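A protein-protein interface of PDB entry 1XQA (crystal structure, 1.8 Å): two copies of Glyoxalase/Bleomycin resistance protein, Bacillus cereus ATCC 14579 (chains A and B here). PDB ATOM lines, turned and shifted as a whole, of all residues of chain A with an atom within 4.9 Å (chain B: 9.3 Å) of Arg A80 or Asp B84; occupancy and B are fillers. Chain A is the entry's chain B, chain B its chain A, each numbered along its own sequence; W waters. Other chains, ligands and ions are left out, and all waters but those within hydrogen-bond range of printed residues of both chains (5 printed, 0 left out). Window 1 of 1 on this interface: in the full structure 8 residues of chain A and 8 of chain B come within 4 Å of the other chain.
Of the 17 printed residues of chain B, 5 touch a printed residue of chain A.
Of the 10 printed residues of chain A, 5 touch a printed residue of chain B.
Among the printed residues, 10 pairs touch across the chains.
Among the printed residues, Asp or Glu carboxylates within 4 Å of a Lys or Arg side-chain nitrogen of the other chain: Lys A76 with Asp B84 (2.8 Å), Arg A80 with Glu B83 (2.8 Å), Arg A80 with Asp B84 (3.0 Å), Glu A83 with Arg B80 (2.9 Å), Asp A84 with Lys B76 (2.8 Å) and Asp A84 with Arg B80 (2.9 Å).
Water W5 lies within hydrogen-bond range of the side-chain carboxylate of Glu A83, the guanidinium group of Arg B80 and the side-chain amide oxygen of Gln B79.
Water W2 lies within hydrogen-bond range of OE1 of Glu B83 (2.6 Å), NE of Arg A80 (2.8 Å) and OE1 of Gln A79 (3.1 Å).
Water W1 lies within hydrogen-bond range of the side-chain carboxylate of Glu A83, the side-chain amide nitrogen of Gln B79 and the side-chain amide nitrogen of Gln A79.
Water W3 bridges NZ of Lys B76 (2.8 Å) and O of Glu A83 (3.4 Å).
Water W4 bridges NZ of Lys A76 (3.0 Å) and O of Glu B83 (3.1 Å).
Of chain B, only Arg B80 (3.5 Å), Glu B83 (2.8 Å) and Asp B84 (3.0 Å) come within 4 Å of Arg A80.
Of chain A, only Lys A76 and Arg A80 come within 4 Å of Asp B84.
Of the printed residues of chain B, Gln A79 touches Gln B79 (3.4 Å).
Printed residues of chain B within 4 Å of Glu A83: Lys B76 (3.7 Å) and Arg B80 (2.9 Å).
Tyr B24 touches none of the printed residues of chain A.
The nearest printed residue of chain A that does not touch Asp B84 is Ile A77 (8.2 Å).
Lys A76 touches Glu B83, and with the chains exchanged Glu A83 touches Lys B76.
Lys A76 touches Asp B84, and with the chains exchanged Asp A84 touches Lys B76.
Gln A79 touches its own counterpart, Gln B79.
Arg A80 touches Glu B83, and with the chains exchanged Glu A83 touches Arg B80.
10 positions are printed for both chains.
The side-chain carboxylate (OD1) of Asp B84 lies within salt-bridge range of the side-chain amino group (NZ) of Lys A76 (2.8 Å).
The guanidinium group of Arg B80 is in salt-bridge range of the side-chain carboxylate of Glu A83, at 2.9 Å.
The guanidinium group (NH2) of Arg B80 is in salt-bridge range of the side-chain carboxylate (OD1) of Asp A84 (2.9 Å).
NZ of Lys A76 is in hydrogen-bond range of O of Glu B83, 3.3 Å away.
NE2 of Gln B79 sits close to NE2 of Gln A79 (3.4 Å).
NZ of Lys B76 lies within salt-bridge range of OD1 of Asp A84.
OE1 of Glu B83 is in salt-bridge range of NH2 of Arg A80 (2.8 Å).
The side-chain carboxylate (OD1) of Asp B84 is in salt-bridge range of the guanidinium group (NH2) of Arg A80, 3.0 Å away.
NE2 of Gln A79 is in hydrogen-bond range of OE2 of Glu A83, 2.8 Å away.
The side-chain hydroxyl (OH) of Tyr B24 is in hydrogen-bond range of the side-chain carboxylate (OD2) of Asp B84, 2.4 Å away.
NE2 of Gln B79 is in hydrogen-bond range of OE2 of Glu B83, at 3.0 Å.
OH of Tyr A24 sits at hydrogen-bond distance from OD2 of Asp A84.
The side-chain amino group of Lys B23 is in salt-bridge range of the side-chain carboxylate of Asp B84.
O of Arg B80 touches NH2 of Arg A80, at 3.5 Å.
Lys B76 touches Glu A83.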
ATOM      1  N   TYR A  24      28.840  10.491  32.070  1.00  0.00           N
ATOM      2  CA  TYR A  24      30.107  10.860  31.471  1.00  0.00           C
ATOM      3  C   TYR A  24      30.744   9.779  30.604  1.00  0.00           C
ATOM      4  O   TYR A  24      31.498  10.105  29.688  1.00  0.00           O
ATOM      5  CB  TYR A  24      31.090  11.406  32.526  1.00  0.00           C
ATOM      6  CG  TYR A  24      30.541  12.642  33.179  1.00  0.00           C
ATOM      7  CD1 TYR A  24      30.612  13.883  32.539  1.00  0.00           C
ATOM      8  CD2 TYR A  24      29.905  12.573  34.419  1.00  0.00           C
ATOM      9  CE1 TYR A  24      30.059  15.032  33.131  1.00  0.00           C
ATOM     10  CE2 TYR A  24      29.366  13.713  35.024  1.00  0.00           C
ATOM     11  CZ  TYR A  24      29.447  14.934  34.374  1.00  0.00           C
ATOM     12  OH  TYR A  24      28.894  16.057  34.960  1.00  0.00           O
ATOM     13  N   LYS A  76      36.515  17.024  25.503  1.00  0.00           N
ATOM     14  CA  LYS A  76      35.088  17.222  25.757  1.00  0.00           C
ATOM     15  C   LYS A  76      34.705  16.741  27.165  1.00  0.00           C
ATOM     16  O   LYS A  76      33.992  17.435  27.900  1.00  0.00           O
ATOM     17  CB  LYS A  76      34.263  16.478  24.699  1.00  0.00           C
ATOM     18  CG  LYS A  76      32.765  16.639  24.833  1.00  0.00           C
ATOM     19  CD  LYS A  76      32.013  15.807  23.781  1.00  0.00           C
ATOM     20  CE  LYS A  76      32.123  16.422  22.389  1.00  0.00           C
ATOM     21  NZ  LYS A  76      31.202  15.750  21.407  1.00  0.00           N
ATOM     22  N   ILE A  77      35.160  15.547  27.531  1.00  0.00           N
ATOM     23  CA  ILE A  77      34.821  14.996  28.832  1.00  0.00           C
ATOM     24  C   ILE A  77      35.468  15.831  29.931  1.00  0.00           C
ATOM     25  O   ILE A  77      34.827  16.150  30.935  1.00  0.00           O
ATOM     26  CB  ILE A  77      35.176  13.491  28.939  1.00  0.00           C
ATOM     27  CG1 ILE A  77      34.370  12.710  27.895  1.00  0.00           C
ATOM     28  CG2 ILE A  77      34.923  12.954  30.377  1.00  0.00           C
ATOM     29  CD1 ILE A  77      34.907  11.284  27.644  1.00  0.00           C
ATOM     30  N   ASN A  78      36.725  16.190  29.719  1.00  0.00           N
ATOM     31  CA  ASN A  78      37.437  17.086  30.641  1.00  0.00           C
ATOM     32  C   ASN A  78      36.670  18.391  30.899  1.00  0.00           C
ATOM     33  O   ASN A  78      36.447  18.763  32.059  1.00  0.00           O
ATOM     34  CB  ASN A  78      38.860  17.344  30.109  1.00  0.00           C
ATOM     35  CG  ASN A  78      39.719  18.105  31.097  1.00  0.00           C
ATOM     36  OD1 ASN A  78      39.772  19.330  31.056  1.00  0.00           O
ATOM     37  ND2 ASN A  78      40.390  17.385  31.998  1.00  0.00           N
ATOM     38  N   GLN A  79      36.282  19.068  29.812  1.00  0.00           N
ATOM     39  CA  GLN A  79      35.528  20.333  29.851  1.00  0.00           C
ATOM     40  C   GLN A  79      34.222  20.210  30.634  1.00  0.00           C
ATOM     41  O   GLN A  79      33.919  21.042  31.493  1.00  0.00           O
ATOM     42  CB  GLN A  79      35.224  20.814  28.417  1.00  0.00           C
ATOM     43  CG  GLN A  79      34.479  22.162  28.306  1.00  0.00           C
ATOM     44  CD  GLN A  79      33.737  22.342  26.979  1.00  0.00           C
ATOM     45  OE1 GLN A  79      34.003  21.647  25.991  1.00  0.00           O
ATOM     46  NE2 GLN A  79      32.798  23.279  26.957  1.00  0.00           N
ATOM     47  N   ARG A  80      33.449  19.177  30.313  1.00  0.00           N
ATOM     48  CA  ARG A  80      32.132  18.981  30.907  1.00  0.00           C
ATOM     49  C   ARG A  80      32.245  18.611  32.382  1.00  0.00           C
ATOM     50  O   ARG A  80      31.478  19.105  33.205  1.00  0.00           O
ATOM     51  CB  ARG A  80      31.335  17.938  30.120  1.00  0.00           C
ATOM     52  CG  ARG A  80      30.942  18.456  28.747  1.00  0.00           C
ATOM     53  CD  ARG A  80      30.314  17.401  27.867  1.00  0.00           C
ATOM     54  NE  ARG A  80      30.089  17.928  26.527  1.00  0.00           N
ATOM     55  CZ  ARG A  80      29.333  17.345  25.605  1.00  0.00           C
ATOM     56  NH1 ARG A  80      28.725  16.182  25.872  1.00  0.00           N
ATOM     57  NH2 ARG A  80      29.214  17.917  24.404  1.00  0.00           N
ATOM     58  N   LEU A  81      33.213  17.768  32.717  1.00  0.00           N
ATOM     59  CA  LEU A  81      33.503  17.500  34.129  1.00  0.00           C
ATOM     60  C   LEU A  81      33.837  18.784  34.900  1.00  0.00           C
ATOM     61  O   LEU A  81      33.261  19.030  35.979  1.00  0.00           O
ATOM     62  CB  LEU A  81      34.614  16.457  34.281  1.00  0.00           C
ATOM     63  CG  LEU A  81      34.254  15.005  33.954  1.00  0.00           C
ATOM     64  CD1 LEU A  81      35.519  14.144  33.861  1.00  0.00           C
ATOM     65  CD2 LEU A  81      33.268  14.416  34.983  1.00  0.00           C
ATOM     66  N   LYS A  82      34.735  19.603  34.342  1.00  0.00           N
ATOM     67  CA  LYS A  82      35.130  20.865  34.966  1.00  0.00           C
ATOM     68  C   LYS A  82      33.913  21.777  35.150  1.00  0.00           C
ATOM     69  O   LYS A  82      33.719  22.340  36.233  1.00  0.00           O
ATOM     70  CB  LYS A  82      36.231  21.574  34.151  1.00  0.00           C
ATOM     71  CG  LYS A  82      36.817  22.837  34.820  1.00  0.00           C
ATOM     72  CD  LYS A  82      38.209  23.169  34.275  1.00  0.00           C
ATOM     73  CE  LYS A  82      39.306  22.490  35.125  1.00  0.00           C
ATOM     74  NZ  LYS A  82      40.739  22.723  34.697  1.00  0.00           N
ATOM     75  N   GLU A  83      33.090  21.899  34.102  1.00  0.00           N
ATOM     76  CA  GLU A  83      31.904  22.765  34.140  1.00  0.00           C
ATOM     77  C   GLU A  83      30.893  22.283  35.163  1.00  0.00           C
ATOM     78  O   GLU A  83      30.213  23.087  35.812  1.00  0.00           O
ATOM     79  CB  GLU A  83      31.224  22.846  32.765  1.00  0.00           C
ATOM     80  CG  GLU A  83      32.007  23.625  31.728  1.00  0.00           C
ATOM     81  CD  GLU A  83      31.392  23.602  30.343  1.00  0.00           C
ATOM     82  OE1 GLU A  83      30.385  22.891  30.109  1.00  0.00           O
ATOM     83  OE2 GLU A  83      31.944  24.303  29.468  1.00  0.00           O
ATOM     84  N   ASP A  84      30.799  20.968  35.303  1.00  0.00           N
ATOM     85  CA  ASP A  84      29.826  20.358  36.183  1.00  0.00           C
ATOM     86  C   ASP A  84      30.297  20.230  37.631  1.00  0.00           C
ATOM     87  O   ASP A  84      29.596  19.646  38.454  1.00  0.00           O
ATOM     88  CB  ASP A  84      29.378  19.014  35.626  1.00  0.00           C
ATOM     89  CG  ASP A  84      28.670  19.141  34.281  1.00  0.00           C
ATOM     90  OD1 ASP A  84      28.385  20.287  33.849  1.00  0.00           O
ATOM     91  OD2 ASP A  84      28.398  18.089  33.658  1.00  0.00           O
ATOM     92  N   PHE B  20      19.589   8.325  25.778  1.00  0.00           N
ATOM     93  CA  PHE B  20      19.490   9.771  25.552  1.00  0.00           C
ATOM     94  C   PHE B  20      18.967  10.482  26.810  1.00  0.00           C
ATOM     95  O   PHE B  20      19.528  11.493  27.250  1.00  0.00           O
ATOM     96  CB  PHE B  20      18.549  10.050  24.375  1.00  0.00           C
ATOM     97  CG  PHE B  20      18.458  11.501  23.995  1.00  0.00           C
ATOM     98  CD1 PHE B  20      19.481  12.096  23.252  1.00  0.00           C
ATOM     99  CD2 PHE B  20      17.336  12.273  24.358  1.00  0.00           C
ATOM    100  CE1 PHE B  20      19.394  13.437  22.869  1.00  0.00           C
ATOM    101  CE2 PHE B  20      17.245  13.624  23.978  1.00  0.00           C
ATOM    102  CZ  PHE B  20      18.288  14.202  23.231  1.00  0.00           C
ATOM    103  N   LYS B  23      21.706  10.351  29.535  1.00  0.00           N
ATOM    104  CA  LYS B  23      22.843  11.220  29.267  1.00  0.00           C
ATOM    105  C   LYS B  23      22.523  12.704  29.424  1.00  0.00           C
ATOM    106  O   LYS B  23      23.250  13.431  30.119  1.00  0.00           O
ATOM    107  CB  LYS B  23      23.383  10.959  27.862  1.00  0.00           C
ATOM    108  CG  LYS B  23      24.700  11.698  27.592  1.00  0.00           C
ATOM    109  CD  LYS B  23      25.306  11.277  26.295  1.00  0.00           C
ATOM    110  CE  LYS B  23      26.580  12.059  26.060  1.00  0.00           C
ATOM    111  NZ  LYS B  23      27.375  11.495  24.919  1.00  0.00           N
ATOM    112  N   TYR B  24      21.438  13.151  28.798  1.00  0.00           N
ATOM    113  CA  TYR B  24      21.152  14.594  28.717  1.00  0.00           C
ATOM    114  C   TYR B  24      20.196  15.128  29.792  1.00  0.00           C
ATOM    115  O   TYR B  24      20.226  16.322  30.129  1.00  0.00           O
ATOM    116  CB  TYR B  24      20.677  14.966  27.301  1.00  0.00           C
ATOM    117  CG  TYR B  24      21.757  14.703  26.284  1.00  0.00           C
ATOM    118  CD1 TYR B  24      22.847  15.575  26.159  1.00  0.00           C
ATOM    119  CD2 TYR B  24      21.734  13.557  25.494  1.00  0.00           C
ATOM    120  CE1 TYR B  24      23.871  15.312  25.259  1.00  0.00           C
ATOM    121  CE2 TYR B  24      22.760  13.291  24.574  1.00  0.00           C
ATOM    122  CZ  TYR B  24      23.818  14.180  24.468  1.00  0.00           C
ATOM    123  OH  TYR B  24      24.821  13.905  23.570  1.00  0.00           O
ATOM    124  N   LYS B  76      23.628  25.277  28.203  1.00  0.00           N
ATOM    125  CA  LYS B  76      24.565  24.174  28.351  1.00  0.00           C
ATOM    126  C   LYS B  76      24.040  22.907  27.661  1.00  0.00           C
ATOM    127  O   LYS B  76      24.775  22.292  26.890  1.00  0.00           O
ATOM    128  CB  LYS B  76      24.876  23.926  29.829  1.00  0.00           C
ATOM    129  CG  LYS B  76      26.240  23.306  30.073  1.00  0.00           C
ATOM    130  CD  LYS B  76      26.786  23.674  31.464  1.00  0.00           C
ATOM    131  CE  LYS B  76      26.479  22.571  32.470  1.00  0.00           C
ATOM    132  NZ  LYS B  76      27.064  22.801  33.836  1.00  0.00           N
ATOM    133  N   ILE B  77      22.782  22.534  27.923  1.00  0.00           N
ATOM    134  CA  ILE B  77      22.191  21.344  27.285  1.00  0.00           C
ATOM    135  C   ILE B  77      22.141  21.502  25.757  1.00  0.00           C
ATOM    136  O   ILE B  77      22.445  20.566  25.000  1.00  0.00           O
ATOM    137  CB  ILE B  77      20.774  21.009  27.838  1.00  0.00           C
ATOM    138  CG1 ILE B  77      20.823  20.717  29.346  1.00  0.00           C
ATOM    139  CG2 ILE B  77      20.186  19.773  27.116  1.00  0.00           C
ATOM    140  CD1 ILE B  77      19.425  20.625  29.997  1.00  0.00           C
ATOM    141  N   ASN B  78      21.715  22.681  25.310  1.00  0.00           N
ATOM    142  CA  ASN B  78      21.742  23.041  23.888  1.00  0.00           C
ATOM    143  C   ASN B  78      23.130  22.856  23.261  1.00  0.00           C
ATOM    144  O   ASN B  78      23.276  22.201  22.235  1.00  0.00           O
ATOM    145  CB  ASN B  78      21.322  24.517  23.753  1.00  0.00           C
ATOM    146  CG  ASN B  78      21.075  24.919  22.319  1.00  0.00           C
ATOM    147  OD1 ASN B  78      21.953  25.490  21.667  1.00  0.00           O
ATOM    148  ND2 ASN B  78      19.883  24.611  21.810  1.00  0.00           N
ATOM    149  N   GLN B  79      24.144  23.452  23.892  1.00  0.00           N
ATOM    150  CA  GLN B  79      25.531  23.379  23.414  1.00  0.00           C
ATOM    151  C   GLN B  79      26.008  21.927  23.347  1.00  0.00           C
ATOM    152  O   GLN B  79      26.596  21.502  22.344  1.00  0.00           O
ATOM    153  CB  GLN B  79      26.459  24.216  24.314  1.00  0.00           C
ATOM    154  CG  GLN B  79      27.963  24.080  24.004  1.00  0.00           C
ATOM    155  CD  GLN B  79      28.899  24.442  25.188  1.00  0.00           C
ATOM    156  OE1 GLN B  79      28.447  24.831  26.283  1.00  0.00           O
ATOM    157  NE2 GLN B  79      30.216  24.306  24.962  1.00  0.00           N
ATOM    158  N   ARG B  80      25.717  21.148  24.388  1.00  0.00           N
ATOM    159  CA  ARG B  80      26.181  19.768  24.422  1.00  0.00           C
ATOM    160  C   ARG B  80      25.485  18.904  23.384  1.00  0.00           C
ATOM    161  O   ARG B  80      26.127  18.076  22.740  1.00  0.00           O
ATOM    162  CB  ARG B  80      26.052  19.177  25.823  1.00  0.00           C
ATOM    163  CG  ARG B  80      27.015  19.833  26.799  1.00  0.00           C
ATOM    164  CD  ARG B  80      26.873  19.346  28.223  1.00  0.00           C
ATOM    165  NE  ARG B  80      27.799  20.111  29.076  1.00  0.00           N
ATOM    166  CZ  ARG B  80      28.062  19.827  30.346  1.00  0.00           C
ATOM    167  NH1 ARG B  80      27.476  18.790  30.949  1.00  0.00           N
ATOM    168  NH2 ARG B  80      28.916  20.578  31.016  1.00  0.00           N
ATOM    169  N   LEU B  81      24.188  19.117  23.208  1.00  0.00           N
ATOM    170  CA  LEU B  81      23.434  18.389  22.165  1.00  0.00           C
ATOM    171  C   LEU B  81      24.007  18.694  20.777  1.00  0.00           C
ATOM    172  O   LEU B  81      24.265  17.782  20.000  1.00  0.00           O
ATOM    173  CB  LEU B  81      21.943  18.725  22.227  1.00  0.00           C
ATOM    174  CG  LEU B  81      21.158  18.084  23.374  1.00  0.00           C
ATOM    175  CD1 LEU B  81      19.760  18.706  23.476  1.00  0.00           C
ATOM    176  CD2 LEU B  81      21.070  16.564  23.202  1.00  0.00           C
ATOM    177  N   LYS B  82      24.239  19.980  20.495  1.00  0.00           N
ATOM    178  CA  LYS B  82      24.841  20.422  19.233  1.00  0.00           C
ATOM    179  C   LYS B  82      26.204  19.766  18.988  1.00  0.00           C
ATOM    180  O   LYS B  82      26.446  19.199  17.914  1.00  0.00           O
ATOM    181  CB  LYS B  82      24.988  21.949  19.223  1.00  0.00           C
ATOM    182  CG  LYS B  82      25.416  22.528  17.869  1.00  0.00           C
ATOM    183  CD  LYS B  82      25.436  24.050  17.903  1.00  0.00           C
ATOM    184  CE  LYS B  82      25.810  24.616  16.544  1.00  0.00           C
ATOM    185  NZ  LYS B  82      26.325  26.015  16.679  1.00  0.00           N
ATOM    186  N   GLU B  83      27.092  19.843  19.981  1.00  0.00           N
ATOM    187  CA  GLU B  83      28.423  19.229  19.884  1.00  0.00           C
ATOM    188  C   GLU B  83      28.378  17.734  19.697  1.00  0.00           C
ATOM    189  O   GLU B  83      29.293  17.153  19.125  1.00  0.00           O
ATOM    190  CB  GLU B  83      29.238  19.498  21.135  1.00  0.00           C
ATOM    191  CG  GLU B  83      29.574  20.940  21.321  1.00  0.00           C
ATOM    192  CD  GLU B  83      30.247  21.202  22.643  1.00  0.00           C
ATOM    193  OE1 GLU B  83      30.280  20.296  23.505  1.00  0.00           O
ATOM    194  OE2 GLU B  83      30.732  22.328  22.814  1.00  0.00           O
ATOM    195  N   ASP B  84      27.327  17.117  20.203  1.00  0.00           N
ATOM    196  CA  ASP B  84      27.185  15.675  20.144  1.00  0.00           C
ATOM    197  C   ASP B  84      26.400  15.217  18.910  1.00  0.00           C
ATOM    198  O   ASP B  84      26.092  14.033  18.768  1.00  0.00           O
ATOM    199  CB  ASP B  84      26.542  15.148  21.429  1.00  0.00           C
ATOM    200  CG  ASP B  84      27.438  15.304  22.645  1.00  0.00           C
ATOM    201  OD1 ASP B  84      28.624  15.718  22.504  1.00  0.00           O
ATOM    202  OD2 ASP B  84      26.951  15.010  23.759  1.00  0.00           O
ATOM    203  N   GLY B  85      26.080  16.154  18.019  1.00  0.00           N
ATOM    204  CA  GLY B  85      25.540  15.795  16.707  1.00  0.00           C
ATOM    205  C   GLY B  85      24.038  15.837  16.563  1.00  0.00           C
ATOM    206  O   GLY B  85      23.499  15.373  15.553  1.00  0.00           O
ATOM    207  N   PHE B  86      23.353  16.381  17.569  1.00  0.00           N
ATOM    208  CA  PHE B  86      21.917  16.599  17.472  1.00  0.00           C
ATOM    209  C   PHE B  86      21.643  17.975  16.870  1.00  0.00           C
ATOM    210  O   PHE B  86      22.345  18.950  17.135  1.00  0.00           O
ATOM    211  CB  PHE B  86      21.224  16.422  18.821  1.00  0.00           C
ATOM    212  CG  PHE B  86      21.360  15.034  19.387  1.00  0.00           C
ATOM    213  CD1 PHE B  86      20.439  14.044  19.068  1.00  0.00           C
ATOM    214  CD2 PHE B  86      22.432  14.709  20.194  1.00  0.00           C
ATOM    215  CE1 PHE B  86      20.578  12.734  19.572  1.00  0.00           C
ATOM    216  CE2 PHE B  86      22.588  13.418  20.710  1.00  0.00           C
ATOM    217  CZ  PHE B  86      21.657  12.426  20.395  1.00  0.00           C
ATOM    218  N   LEU B  87      20.607  18.037  16.054  1.00  0.00           N
ATOM    219  CA  LEU B  87      20.278  19.262  15.346  1.00  0.00           C
ATOM    220  C   LEU B  87      19.389  20.148  16.218  1.00  0.00           C
ATOM    221  O   LEU B  87      18.208  19.881  16.454  1.00  0.00           O
ATOM    222  CB  LEU B  87      19.670  18.937  13.979  1.00  0.00           C
ATOM    223  CG  LEU B  87      20.409  17.877  13.143  1.00  0.00           C
ATOM    224  CD1 LEU B  87      19.724  17.696  11.786  1.00  0.00           C
ATOM    225  CD2 LEU B  87      21.911  18.166  12.941  1.00  0.00           C
ATOM    226  N   VAL B  88      19.992  21.181  16.772  1.00  0.00           N
ATOM    227  CA  VAL B  88      19.256  22.085  17.628  1.00  0.00           C
ATOM    228  C   VAL B  88      19.575  23.485  17.168  1.00  0.00           C
ATOM    229  O   VAL B  88      20.677  23.741  16.665  1.00  0.00           O
ATOM    230  CB  VAL B  88      19.627  21.908  19.131  1.00  0.00           C
ATOM    231  CG1 VAL B  88      19.083  20.585  19.676  1.00  0.00           C
ATOM    232  CG2 VAL B  88      21.133  21.987  19.341  1.00  0.00           C
ATOM    233  N   PRO B 104      15.889  10.584  20.213  1.00  0.00           N
ATOM    234  CA  PRO B 104      15.905   9.166  19.867  1.00  0.00           C
ATOM    235  C   PRO B 104      14.625   8.481  20.344  1.00  0.00           C
ATOM    236  O   PRO B 104      14.152   8.744  21.464  1.00  0.00           O
ATOM    237  CB  PRO B 104      17.123   8.637  20.626  1.00  0.00           C
ATOM    238  CG  PRO B 104      18.084   9.803  20.614  1.00  0.00           C
ATOM    239  CD  PRO B 104      17.160  11.000  20.845  1.00  0.00           C
HETATM  240  O   HOH W   1      31.127  25.516  27.261  1.00  0.00           O
HETATM  241  O   HOH W   2      31.080  20.537  25.998  1.00  0.00           O
HETATM  242  O   HOH W   3      28.339  25.295  33.948  1.00  0.00           O
HETATM  243  O   HOH W   4      32.393  17.173  19.054  1.00  0.00           O
HETATM  244  O   HOH W   5      29.454  22.127  27.854  1.00  0.00           O
